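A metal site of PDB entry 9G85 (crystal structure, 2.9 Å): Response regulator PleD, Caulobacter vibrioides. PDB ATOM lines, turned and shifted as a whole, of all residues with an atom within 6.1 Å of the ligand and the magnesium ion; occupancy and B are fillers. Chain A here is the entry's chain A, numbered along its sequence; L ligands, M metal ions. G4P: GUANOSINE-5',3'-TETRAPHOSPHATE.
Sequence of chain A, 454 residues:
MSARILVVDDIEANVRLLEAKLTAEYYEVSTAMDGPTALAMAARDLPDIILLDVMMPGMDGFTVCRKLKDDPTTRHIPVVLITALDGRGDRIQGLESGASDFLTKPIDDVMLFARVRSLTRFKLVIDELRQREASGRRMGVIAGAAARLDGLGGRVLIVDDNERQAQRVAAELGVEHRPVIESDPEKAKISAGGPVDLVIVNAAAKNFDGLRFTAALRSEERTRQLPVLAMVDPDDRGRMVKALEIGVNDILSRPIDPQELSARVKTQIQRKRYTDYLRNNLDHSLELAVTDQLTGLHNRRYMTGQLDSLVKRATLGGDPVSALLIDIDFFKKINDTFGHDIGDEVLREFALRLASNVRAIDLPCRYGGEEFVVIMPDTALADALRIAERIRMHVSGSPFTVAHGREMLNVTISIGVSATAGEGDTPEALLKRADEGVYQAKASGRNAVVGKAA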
ATOM      1  N   LEU A 294      17.122 -10.141  26.702  1.00  0.00           N
ATOM      2  CA  LEU A 294      17.124  -8.677  26.766  1.00  0.00           C
ATOM      3  C   LEU A 294      16.106  -8.081  25.796  1.00  0.00           C
ATOM      4  O   LEU A 294      15.173  -7.384  26.205  1.00  0.00           O
ATOM      5  CB  LEU A 294      18.538  -8.149  26.459  1.00  0.00           C
ATOM      6  CG  LEU A 294      18.718  -6.635  26.399  1.00  0.00           C
ATOM      7  CD1 LEU A 294      18.743  -6.020  27.794  1.00  0.00           C
ATOM      8  CD2 LEU A 294      19.978  -6.270  25.634  1.00  0.00           C
ATOM      9  N   ASP A 327      23.503  -3.507  11.518  1.00  0.00           N
ATOM     10  CA  ASP A 327      24.501  -3.218  12.537  1.00  0.00           C
ATOM     11  C   ASP A 327      24.370  -1.760  12.955  1.00  0.00           C
ATOM     12  O   ASP A 327      24.349  -0.868  12.114  1.00  0.00           O
ATOM     13  CB  ASP A 327      25.917  -3.498  12.028  1.00  0.00           C
ATOM     14  CG  ASP A 327      26.949  -3.525  13.129  1.00  0.00           C
ATOM     15  OD1 ASP A 327      27.167  -4.611  13.702  1.00  0.00           O
ATOM     16  OD2 ASP A 327      27.536  -2.457  13.431  1.00  0.00           O
ATOM     17  N   ILE A 328      24.287  -1.524  14.271  1.00  0.00           N
ATOM     18  CA  ILE A 328      24.116  -0.165  14.787  1.00  0.00           C
ATOM     19  C   ILE A 328      25.434   0.584  14.739  1.00  0.00           C
ATOM     20  O   ILE A 328      26.483   0.057  15.150  1.00  0.00           O
ATOM     21  CB  ILE A 328      23.552  -0.203  16.215  1.00  0.00           C
ATOM     22  CG1 ILE A 328      22.249  -1.014  16.250  1.00  0.00           C
ATOM     23  CG2 ILE A 328      23.312   1.209  16.736  1.00  0.00           C
ATOM     24  CD1 ILE A 328      21.627  -1.117  17.630  1.00  0.00           C
ATOM     25  N   ASP A 329      25.404   1.820  14.250  1.00  0.00           N
ATOM     26  CA  ASP A 329      26.610   2.624  14.087  1.00  0.00           C
ATOM     27  C   ASP A 329      26.969   3.322  15.397  1.00  0.00           C
ATOM     28  O   ASP A 329      26.101   3.931  16.036  1.00  0.00           O
ATOM     29  CB  ASP A 329      26.424   3.660  12.986  1.00  0.00           C
ATOM     30  CG  ASP A 329      26.098   3.049  11.644  1.00  0.00           C
ATOM     31  OD1 ASP A 329      26.626   1.951  11.355  1.00  0.00           O
ATOM     32  OD2 ASP A 329      25.333   3.661  10.880  1.00  0.00           O
ATOM     33  N   PHE A 330      28.235   3.210  15.787  1.00  0.00           N
ATOM     34  CA  PHE A 330      28.784   3.933  16.943  1.00  0.00           C
ATOM     35  C   PHE A 330      28.064   3.563  18.239  1.00  0.00           C
ATOM     36  O   PHE A 330      27.662   4.427  19.012  1.00  0.00           O
ATOM     37  CB  PHE A 330      28.719   5.451  16.714  1.00  0.00           C
ATOM     38  CG  PHE A 330      29.284   5.888  15.397  1.00  0.00           C
ATOM     39  CD1 PHE A 330      30.510   5.421  14.950  1.00  0.00           C
ATOM     40  CD2 PHE A 330      28.582   6.771  14.599  1.00  0.00           C
ATOM     41  CE1 PHE A 330      31.018   5.830  13.738  1.00  0.00           C
ATOM     42  CE2 PHE A 330      29.082   7.186  13.378  1.00  0.00           C
ATOM     43  CZ  PHE A 330      30.312   6.708  12.953  1.00  0.00           C
ATOM     44  N   PHE A 331      27.916   2.261  18.480  1.00  0.00           N
ATOM     45  CA  PHE A 331      27.241   1.843  19.700  1.00  0.00           C
ATOM     46  C   PHE A 331      28.130   2.006  20.925  1.00  0.00           C
ATOM     47  O   PHE A 331      27.617   2.231  22.029  1.00  0.00           O
ATOM     48  CB  PHE A 331      26.762   0.395  19.586  1.00  0.00           C
ATOM     49  CG  PHE A 331      25.668   0.052  20.560  1.00  0.00           C
ATOM     50  CD1 PHE A 331      24.336   0.285  20.237  1.00  0.00           C
ATOM     51  CD2 PHE A 331      25.973  -0.451  21.816  1.00  0.00           C
ATOM     52  CE1 PHE A 331      23.330  -0.008  21.143  1.00  0.00           C
ATOM     53  CE2 PHE A 331      24.974  -0.756  22.719  1.00  0.00           C
ATOM     54  CZ  PHE A 331      23.643  -0.533  22.376  1.00  0.00           C
ATOM     55  N   LYS A 332      29.452   1.895  20.753  1.00  0.00           N
ATOM     56  CA  LYS A 332      30.360   2.136  21.863  1.00  0.00           C
ATOM     57  C   LYS A 332      30.160   3.516  22.466  1.00  0.00           C
ATOM     58  O   LYS A 332      30.153   3.674  23.689  1.00  0.00           O
ATOM     59  CB  LYS A 332      31.816   1.966  21.408  1.00  0.00           C
ATOM     60  CG  LYS A 332      32.148   0.560  20.908  1.00  0.00           C
ATOM     61  CD  LYS A 332      33.602   0.458  20.432  1.00  0.00           C
ATOM     62  CE  LYS A 332      33.933  -0.962  19.991  1.00  0.00           C
ATOM     63  N   LYS A 333      29.982   4.536  21.613  1.00  0.00           N
ATOM     64  CA  LYS A 333      29.793   5.897  22.115  1.00  0.00           C
ATOM     65  C   LYS A 333      28.558   6.009  22.984  1.00  0.00           C
ATOM     66  O   LYS A 333      28.534   6.773  23.961  1.00  0.00           O
ATOM     67  CB  LYS A 333      29.707   6.884  20.949  1.00  0.00           C
ATOM     68  CG  LYS A 333      30.558   6.527  19.737  1.00  0.00           C
ATOM     69  N   ASN A 335      27.346   3.556  24.941  1.00  0.00           N
ATOM     70  CA  ASN A 335      27.772   3.009  26.223  1.00  0.00           C
ATOM     71  C   ASN A 335      28.715   3.954  26.945  1.00  0.00           C
ATOM     72  O   ASN A 335      28.671   4.078  28.173  1.00  0.00           O
ATOM     73  CB  ASN A 335      28.445   1.649  26.015  1.00  0.00           C
ATOM     74  CG  ASN A 335      27.453   0.574  25.633  1.00  0.00           C
ATOM     75  OD1 ASN A 335      26.343   0.519  26.146  1.00  0.00           O
ATOM     76  ND2 ASN A 335      27.859  -0.304  24.725  1.00  0.00           N
ATOM     77  N   ASP A 336      29.565   4.657  26.194  1.00  0.00           N
ATOM     78  CA  ASP A 336      30.526   5.580  26.808  1.00  0.00           C
ATOM     79  C   ASP A 336      29.827   6.788  27.397  1.00  0.00           C
ATOM     80  O   ASP A 336      30.088   7.166  28.545  1.00  0.00           O
ATOM     81  CB  ASP A 336      31.549   6.027  25.763  1.00  0.00           C
ATOM     82  CG  ASP A 336      32.505   4.925  25.379  1.00  0.00           C
ATOM     83  OD1 ASP A 336      32.453   3.849  26.010  1.00  0.00           O
ATOM     84  OD2 ASP A 336      33.296   5.139  24.441  1.00  0.00           O
ATOM     85  N   GLY A 339      26.208   5.098  29.487  1.00  0.00           N
ATOM     86  CA  GLY A 339      26.343   3.928  30.343  1.00  0.00           C
ATOM     87  C   GLY A 339      25.780   2.684  29.684  1.00  0.00           C
ATOM     88  O   GLY A 339      25.051   2.726  28.694  1.00  0.00           O
ATOM     89  N   HIS A 340      26.132   1.544  30.284  1.00  0.00           N
ATOM     90  CA  HIS A 340      25.767   0.265  29.701  1.00  0.00           C
ATOM     91  C   HIS A 340      24.277  -0.022  29.854  1.00  0.00           C
ATOM     92  O   HIS A 340      23.695  -0.716  29.014  1.00  0.00           O
ATOM     93  CB  HIS A 340      26.598  -0.859  30.323  1.00  0.00           C
ATOM     94  CG  HIS A 340      26.775  -2.052  29.433  1.00  0.00           C
ATOM     95  ND1 HIS A 340      25.984  -3.172  29.537  1.00  0.00           N
ATOM     96  CD2 HIS A 340      27.645  -2.298  28.429  1.00  0.00           C
ATOM     97  CE1 HIS A 340      26.354  -4.061  28.636  1.00  0.00           C
ATOM     98  NE2 HIS A 340      27.370  -3.550  27.947  1.00  0.00           N
ATOM     99  N   ASP A 341      23.650   0.489  30.914  1.00  0.00           N
ATOM    100  CA  ASP A 341      22.226   0.236  31.122  1.00  0.00           C
ATOM    101  C   ASP A 341      21.373   0.985  30.115  1.00  0.00           C
ATOM    102  O   ASP A 341      20.354   0.467  29.633  1.00  0.00           O
ATOM    103  CB  ASP A 341      21.826   0.606  32.548  1.00  0.00           C
ATOM    104  CG  ASP A 341      22.313  -0.394  33.565  1.00  0.00           C
ATOM    105  OD1 ASP A 341      22.957  -1.384  33.161  1.00  0.00           O
ATOM    106  OD2 ASP A 341      22.051  -0.203  34.780  1.00  0.00           O
ATOM    107  N   ILE A 342      21.758   2.222  29.781  1.00  0.00           N
ATOM    108  CA  ILE A 342      21.048   2.952  28.738  1.00  0.00           C
ATOM    109  C   ILE A 342      21.278   2.289  27.386  1.00  0.00           C
ATOM    110  O   ILE A 342      20.368   2.225  26.543  1.00  0.00           O
ATOM    111  CB  ILE A 342      21.477   4.430  28.724  1.00  0.00           C
ATOM    112  CG1 ILE A 342      21.054   5.117  30.023  1.00  0.00           C
ATOM    113  CG2 ILE A 342      20.884   5.157  27.528  1.00  0.00           C
ATOM    114  CD1 ILE A 342      19.634   4.807  30.443  1.00  0.00           C
ATOM    115  N   GLY A 343      22.488   1.778  27.158  1.00  0.00           N
ATOM    116  CA  GLY A 343      22.741   0.984  25.962  1.00  0.00           C
ATOM    117  C   GLY A 343      21.777  -0.179  25.837  1.00  0.00           C
ATOM    118  O   GLY A 343      21.284  -0.480  24.741  1.00  0.00           O
ATOM    119  N   ASP A 344      21.496  -0.858  26.955  1.00  0.00           N
ATOM    120  CA  ASP A 344      20.528  -1.949  26.924  1.00  0.00           C
ATOM    121  C   ASP A 344      19.121  -1.447  26.629  1.00  0.00           C
ATOM    122  O   ASP A 344      18.342  -2.151  25.971  1.00  0.00           O
ATOM    123  CB  ASP A 344      20.564  -2.705  28.257  1.00  0.00           C
ATOM    124  CG  ASP A 344      21.878  -3.435  28.478  1.00  0.00           C
ATOM    125  OD1 ASP A 344      22.830  -3.180  27.723  1.00  0.00           O
ATOM    126  OD2 ASP A 344      21.954  -4.260  29.417  1.00  0.00           O
ATOM    127  N   LEU A 347      18.901  -1.022  22.876  1.00  0.00           N
ATOM    128  CA  LEU A 347      18.739  -2.301  22.197  1.00  0.00           C
ATOM    129  C   LEU A 347      17.297  -2.807  22.293  1.00  0.00           C
ATOM    130  O   LEU A 347      16.764  -3.342  21.319  1.00  0.00           O
ATOM    131  CB  LEU A 347      19.708  -3.338  22.769  1.00  0.00           C
ATOM    132  CG  LEU A 347      21.191  -3.160  22.454  1.00  0.00           C
ATOM    133  CD1 LEU A 347      21.990  -4.262  23.123  1.00  0.00           C
ATOM    134  CD2 LEU A 347      21.446  -3.158  20.961  1.00  0.00           C
ATOM    135  N   ARG A 366      18.195 -11.365  16.996  1.00  0.00           N
ATOM    136  CA  ARG A 366      19.429 -10.743  17.472  1.00  0.00           C
ATOM    137  C   ARG A 366      20.579 -11.651  17.039  1.00  0.00           C
ATOM    138  O   ARG A 366      20.738 -12.759  17.557  1.00  0.00           O
ATOM    139  CB  ARG A 366      19.404 -10.558  18.984  1.00  0.00           C
ATOM    140  CG  ARG A 366      20.558  -9.705  19.478  1.00  0.00           C
ATOM    141  CD  ARG A 366      20.573  -9.589  20.983  1.00  0.00           C
ATOM    142  NE  ARG A 366      21.746  -8.851  21.428  1.00  0.00           N
ATOM    143  CZ  ARG A 366      21.967  -8.478  22.680  1.00  0.00           C
ATOM    144  NH1 ARG A 366      21.143  -8.812  23.653  1.00  0.00           N
ATOM    145  NH2 ARG A 366      23.062  -7.769  22.955  1.00  0.00           N
ATOM    146  N   GLY A 368      24.162 -10.772  16.638  1.00  0.00           N
ATOM    147  CA  GLY A 368      25.357 -10.574  17.432  1.00  0.00           C
ATOM    148  C   GLY A 368      25.048  -9.744  18.664  1.00  0.00           C
ATOM    149  O   GLY A 368      23.943  -9.759  19.187  1.00  0.00           O
ATOM    150  N   GLY A 369      26.064  -9.013  19.120  1.00  0.00           N
ATOM    151  CA  GLY A 369      25.872  -8.126  20.249  1.00  0.00           C
ATOM    152  C   GLY A 369      24.922  -7.002  19.922  1.00  0.00           C
ATOM    153  O   GLY A 369      23.814  -6.930  20.482  1.00  0.00           O
ATOM    154  N   GLU A 370      25.320  -6.124  19.012  1.00  0.00           N
ATOM    155  CA  GLU A 370      24.466  -5.059  18.519  1.00  0.00           C
ATOM    156  C   GLU A 370      24.136  -5.230  17.044  1.00  0.00           C
ATOM    157  O   GLU A 370      23.825  -4.263  16.346  1.00  0.00           O
ATOM    158  CB  GLU A 370      25.113  -3.693  18.773  1.00  0.00           C
ATOM    159  CG  GLU A 370      26.586  -3.602  18.402  1.00  0.00           C
ATOM    160  CD  GLU A 370      26.833  -3.603  16.904  1.00  0.00           C
ATOM    161  OE1 GLU A 370      26.185  -2.804  16.197  1.00  0.00           O
ATOM    162  OE2 GLU A 370      27.675  -4.394  16.438  1.00  0.00           O
ATOM    163  N   LYS A 442      29.721   0.064   5.987  1.00  0.00           N
ATOM    164  CA  LYS A 442      30.488   0.734   7.031  1.00  0.00           C
ATOM    165  C   LYS A 442      31.659   1.517   6.449  1.00  0.00           C
ATOM    166  O   LYS A 442      31.992   2.604   6.932  1.00  0.00           O
ATOM    167  CB  LYS A 442      30.999  -0.281   8.059  1.00  0.00           C
ATOM    168  CG  LYS A 442      29.932  -1.027   8.825  1.00  0.00           C
ATOM    169  CD  LYS A 442      29.313  -0.174   9.910  1.00  0.00           C
ATOM    170  CE  LYS A 442      28.305  -0.983  10.720  1.00  0.00           C
ATOM    171  NZ  LYS A 442      27.679  -0.201  11.822  1.00  0.00           N
ATOM    172  N   ARG A 446      28.406   5.887   6.884  1.00  0.00           N
ATOM    173  CA  ARG A 446      27.476   5.171   7.729  1.00  0.00           C
ATOM    174  C   ARG A 446      26.060   5.430   7.231  1.00  0.00           C
ATOM    175  O   ARG A 446      25.841   6.221   6.316  1.00  0.00           O
ATOM    176  CB  ARG A 446      27.611   5.572   9.196  1.00  0.00           C
ATOM    177  CG  ARG A 446      28.946   5.200   9.835  1.00  0.00           C
ATOM    178  CD  ARG A 446      29.135   3.691   9.911  1.00  0.00           C
ATOM    179  NE  ARG A 446      30.520   3.321  10.205  1.00  0.00           N
ATOM    180  CZ  ARG A 446      30.966   2.996  11.409  1.00  0.00           C
ATOM    181  NH1 ARG A 446      30.170   2.983  12.471  1.00  0.00           N
ATOM    182  NH2 ARG A 446      32.251   2.663  11.552  1.00  0.00           N
HETATM  183  PB  G4P L   1      30.298   0.131  16.216  1.00  0.00           P
HETATM  184  O1B G4P L   1      31.026   1.114  15.326  1.00  0.00           O
HETATM  185  O2B G4P L   1      29.799   0.833  17.469  1.00  0.00           O
HETATM  186  O3B G4P L   1      29.140  -0.362  15.393  1.00  0.00           O
HETATM  187  O3A G4P L   1      31.221  -1.158  16.706  1.00  0.00           O
HETATM  188  PA  G4P L   1      30.502  -2.428  17.478  1.00  0.00           P
HETATM  189  O1A G4P L   1      30.348  -3.617  16.540  1.00  0.00           O
HETATM  190  O2A G4P L   1      29.137  -1.887  17.872  1.00  0.00           O
HETATM  191  O5' G4P L   1      31.286  -2.878  18.869  1.00  0.00           O
HETATM  192  C5' G4P L   1      30.776  -3.930  19.680  1.00  0.00           C
HETATM  193  C4' G4P L   1      29.799  -3.359  20.693  1.00  0.00           C
HETATM  194  O4' G4P L   1      28.682  -3.986  20.769  1.00  0.00           O
HETATM  195  C3' G4P L   1      30.465  -3.449  22.223  1.00  0.00           C
HETATM  196  O3' G4P L   1      31.635  -2.505  22.373  1.00  0.00           O
HETATM  197  C2' G4P L   1      29.532  -3.159  22.955  1.00  0.00           C
HETATM  198  O2' G4P L   1      29.535  -1.698  23.294  1.00  0.00           O
HETATM  199  C1' G4P L   1      28.196  -3.392  22.094  1.00  0.00           C
HETATM  200  N9  G4P L   1      27.312  -4.039  22.848  1.00  0.00           N
HETATM  201  C8  G4P L   1      27.381  -5.272  22.307  1.00  0.00           C
HETATM  202  N7  G4P L   1      26.476  -6.033  23.022  1.00  0.00           N
HETATM  203  C5  G4P L   1      25.903  -5.239  23.945  1.00  0.00           C
HETATM  204  C6  G4P L   1      24.842  -5.406  25.054  1.00  0.00           C
HETATM  205  O6  G4P L   1      24.330  -6.471  25.219  1.00  0.00           O
HETATM  206  N1  G4P L   1      24.435  -4.316  25.912  1.00  0.00           N
HETATM  207  C2  G4P L   1      25.026  -3.016  25.729  1.00  0.00           C
HETATM  208  N2  G4P L   1      24.708  -1.842  26.517  1.00  0.00           N
HETATM  209  N3  G4P L   1      26.039  -2.858  24.696  1.00  0.00           N
HETATM  210  C4  G4P L   1      26.447  -3.991  23.820  1.00  0.00           C
HETATM  211  PC  G4P L   1      32.328  -2.250  23.888  1.00  0.00           P
HETATM  212  O1C G4P L   1      33.847  -2.267  23.820  1.00  0.00           O
HETATM  213  O2C G4P L   1      31.876  -0.901  24.384  1.00  0.00           O
HETATM  214  O3C G4P L   1      31.758  -3.409  24.957  1.00  0.00           O
HETATM  215  PD  G4P L   1      30.972  -2.996  26.370  1.00  0.00           P
HETATM  216  O1D G4P L   1      30.217  -4.181  26.947  1.00  0.00           O
HETATM  217  O2D G4P L   1      30.005  -1.878  26.036  1.00  0.00           O
HETATM  218  O3D G4P L   1      31.985  -2.505  27.382  1.00  0.00           O
HETATM  219 MG    MG M   1      27.829  -1.703  15.307  1.00  0.00          MG
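Residues that only touch the ligand: Gly 343, Gly 369 and Leu 347. Hydrophobic or aromatic side chains that line the ligand: Phe 331, His 340 and Leu 347. 15 residues have an atom within 4 Å of the ligand: Asp 327, Ile 328, Phe 330, Phe 331, Lys 332, Asn 335, His 340, Gly 343, Asp 344, Leu 347, Arg 366, Gly 369, Glu 370, Lys 442 and Arg 446. Along chain A the residues within 4 Å of the ligand span positions 327 to 446.
Merely in contact with the magnesium ion: Lys 442 (3.8 Å). Within 4 Å of the magnesium ion: Asp 327, Ile 328, Glu 370 and Lys 442. The nearest printed residue that does not touch the magnesium ion is Asp 329 (4.4 Å).
O of Gly 369 lies within hydrogen-bond range of NH2 of Arg 366, 2.7 Å away. The side-chain amino group (NZ) of Lys 442 lies within hydrogen-bond range of the backbone carbonyl oxygen (O) of Asp 327. NE of Arg 366 sits at hydrogen-bond distance from O of Gly 368 (3.3 Å). OD1 of Asp 329 is in salt-bridge range of NH1 of Arg 446 (3.9 Å). The side-chain carboxylate of Asp 329 is in salt-bridge range of the side-chain amino group of Lys 442 (2.4 Å).
NZ of Lys 442 lies close to O3B of the ligand. The side-chain carboxylate (OD1) of Asp 344 is in hydrogen-bond range of a nitrogen (N2) of the ligand (2.6 Å). The guanidinium group (NH2) of Arg 366 sits at hydrogen-bond distance from an oxygen (O6) of the ligand, 2.9 Å away. The guanidinium group (NH1) of Arg 446 is in salt-bridge range of an oxygen (O1B) of the ligand. The backbone NH (N) of Phe 331 is in hydrogen-bond range of an oxygen (O2B) of the ligand, 2.6 Å away. O of His 340 is in hydrogen-bond range of N2 of the ligand, 2.9 Å away. O2B of the ligand lies within hydrogen-bond range of N of Lys 332, 3.5 Å away. An oxygen (O2B) of the ligand sits close to the backbone NH (N) of Phe 330 (3.3 Å). An oxygen (O1D) of the ligand lies within hydrogen-bond range of a ring nitrogen (NE2) of His 340 (3.1 Å). ND2 of Asn 335 sits at hydrogen-bond distance from O2' of the ligand (2.6 Å).
O3B of the ligand is bound to the magnesium ion (1.9 Å). OD2 of Asp 327 is bound to the magnesium ion, at 2.0 Å. OE1 of Glu 370 is bound to the magnesium ion (2.2 Å). The magnesium ion is bound by the backbone carbonyl oxygen (O) of Ile 328 (2.2 Å).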
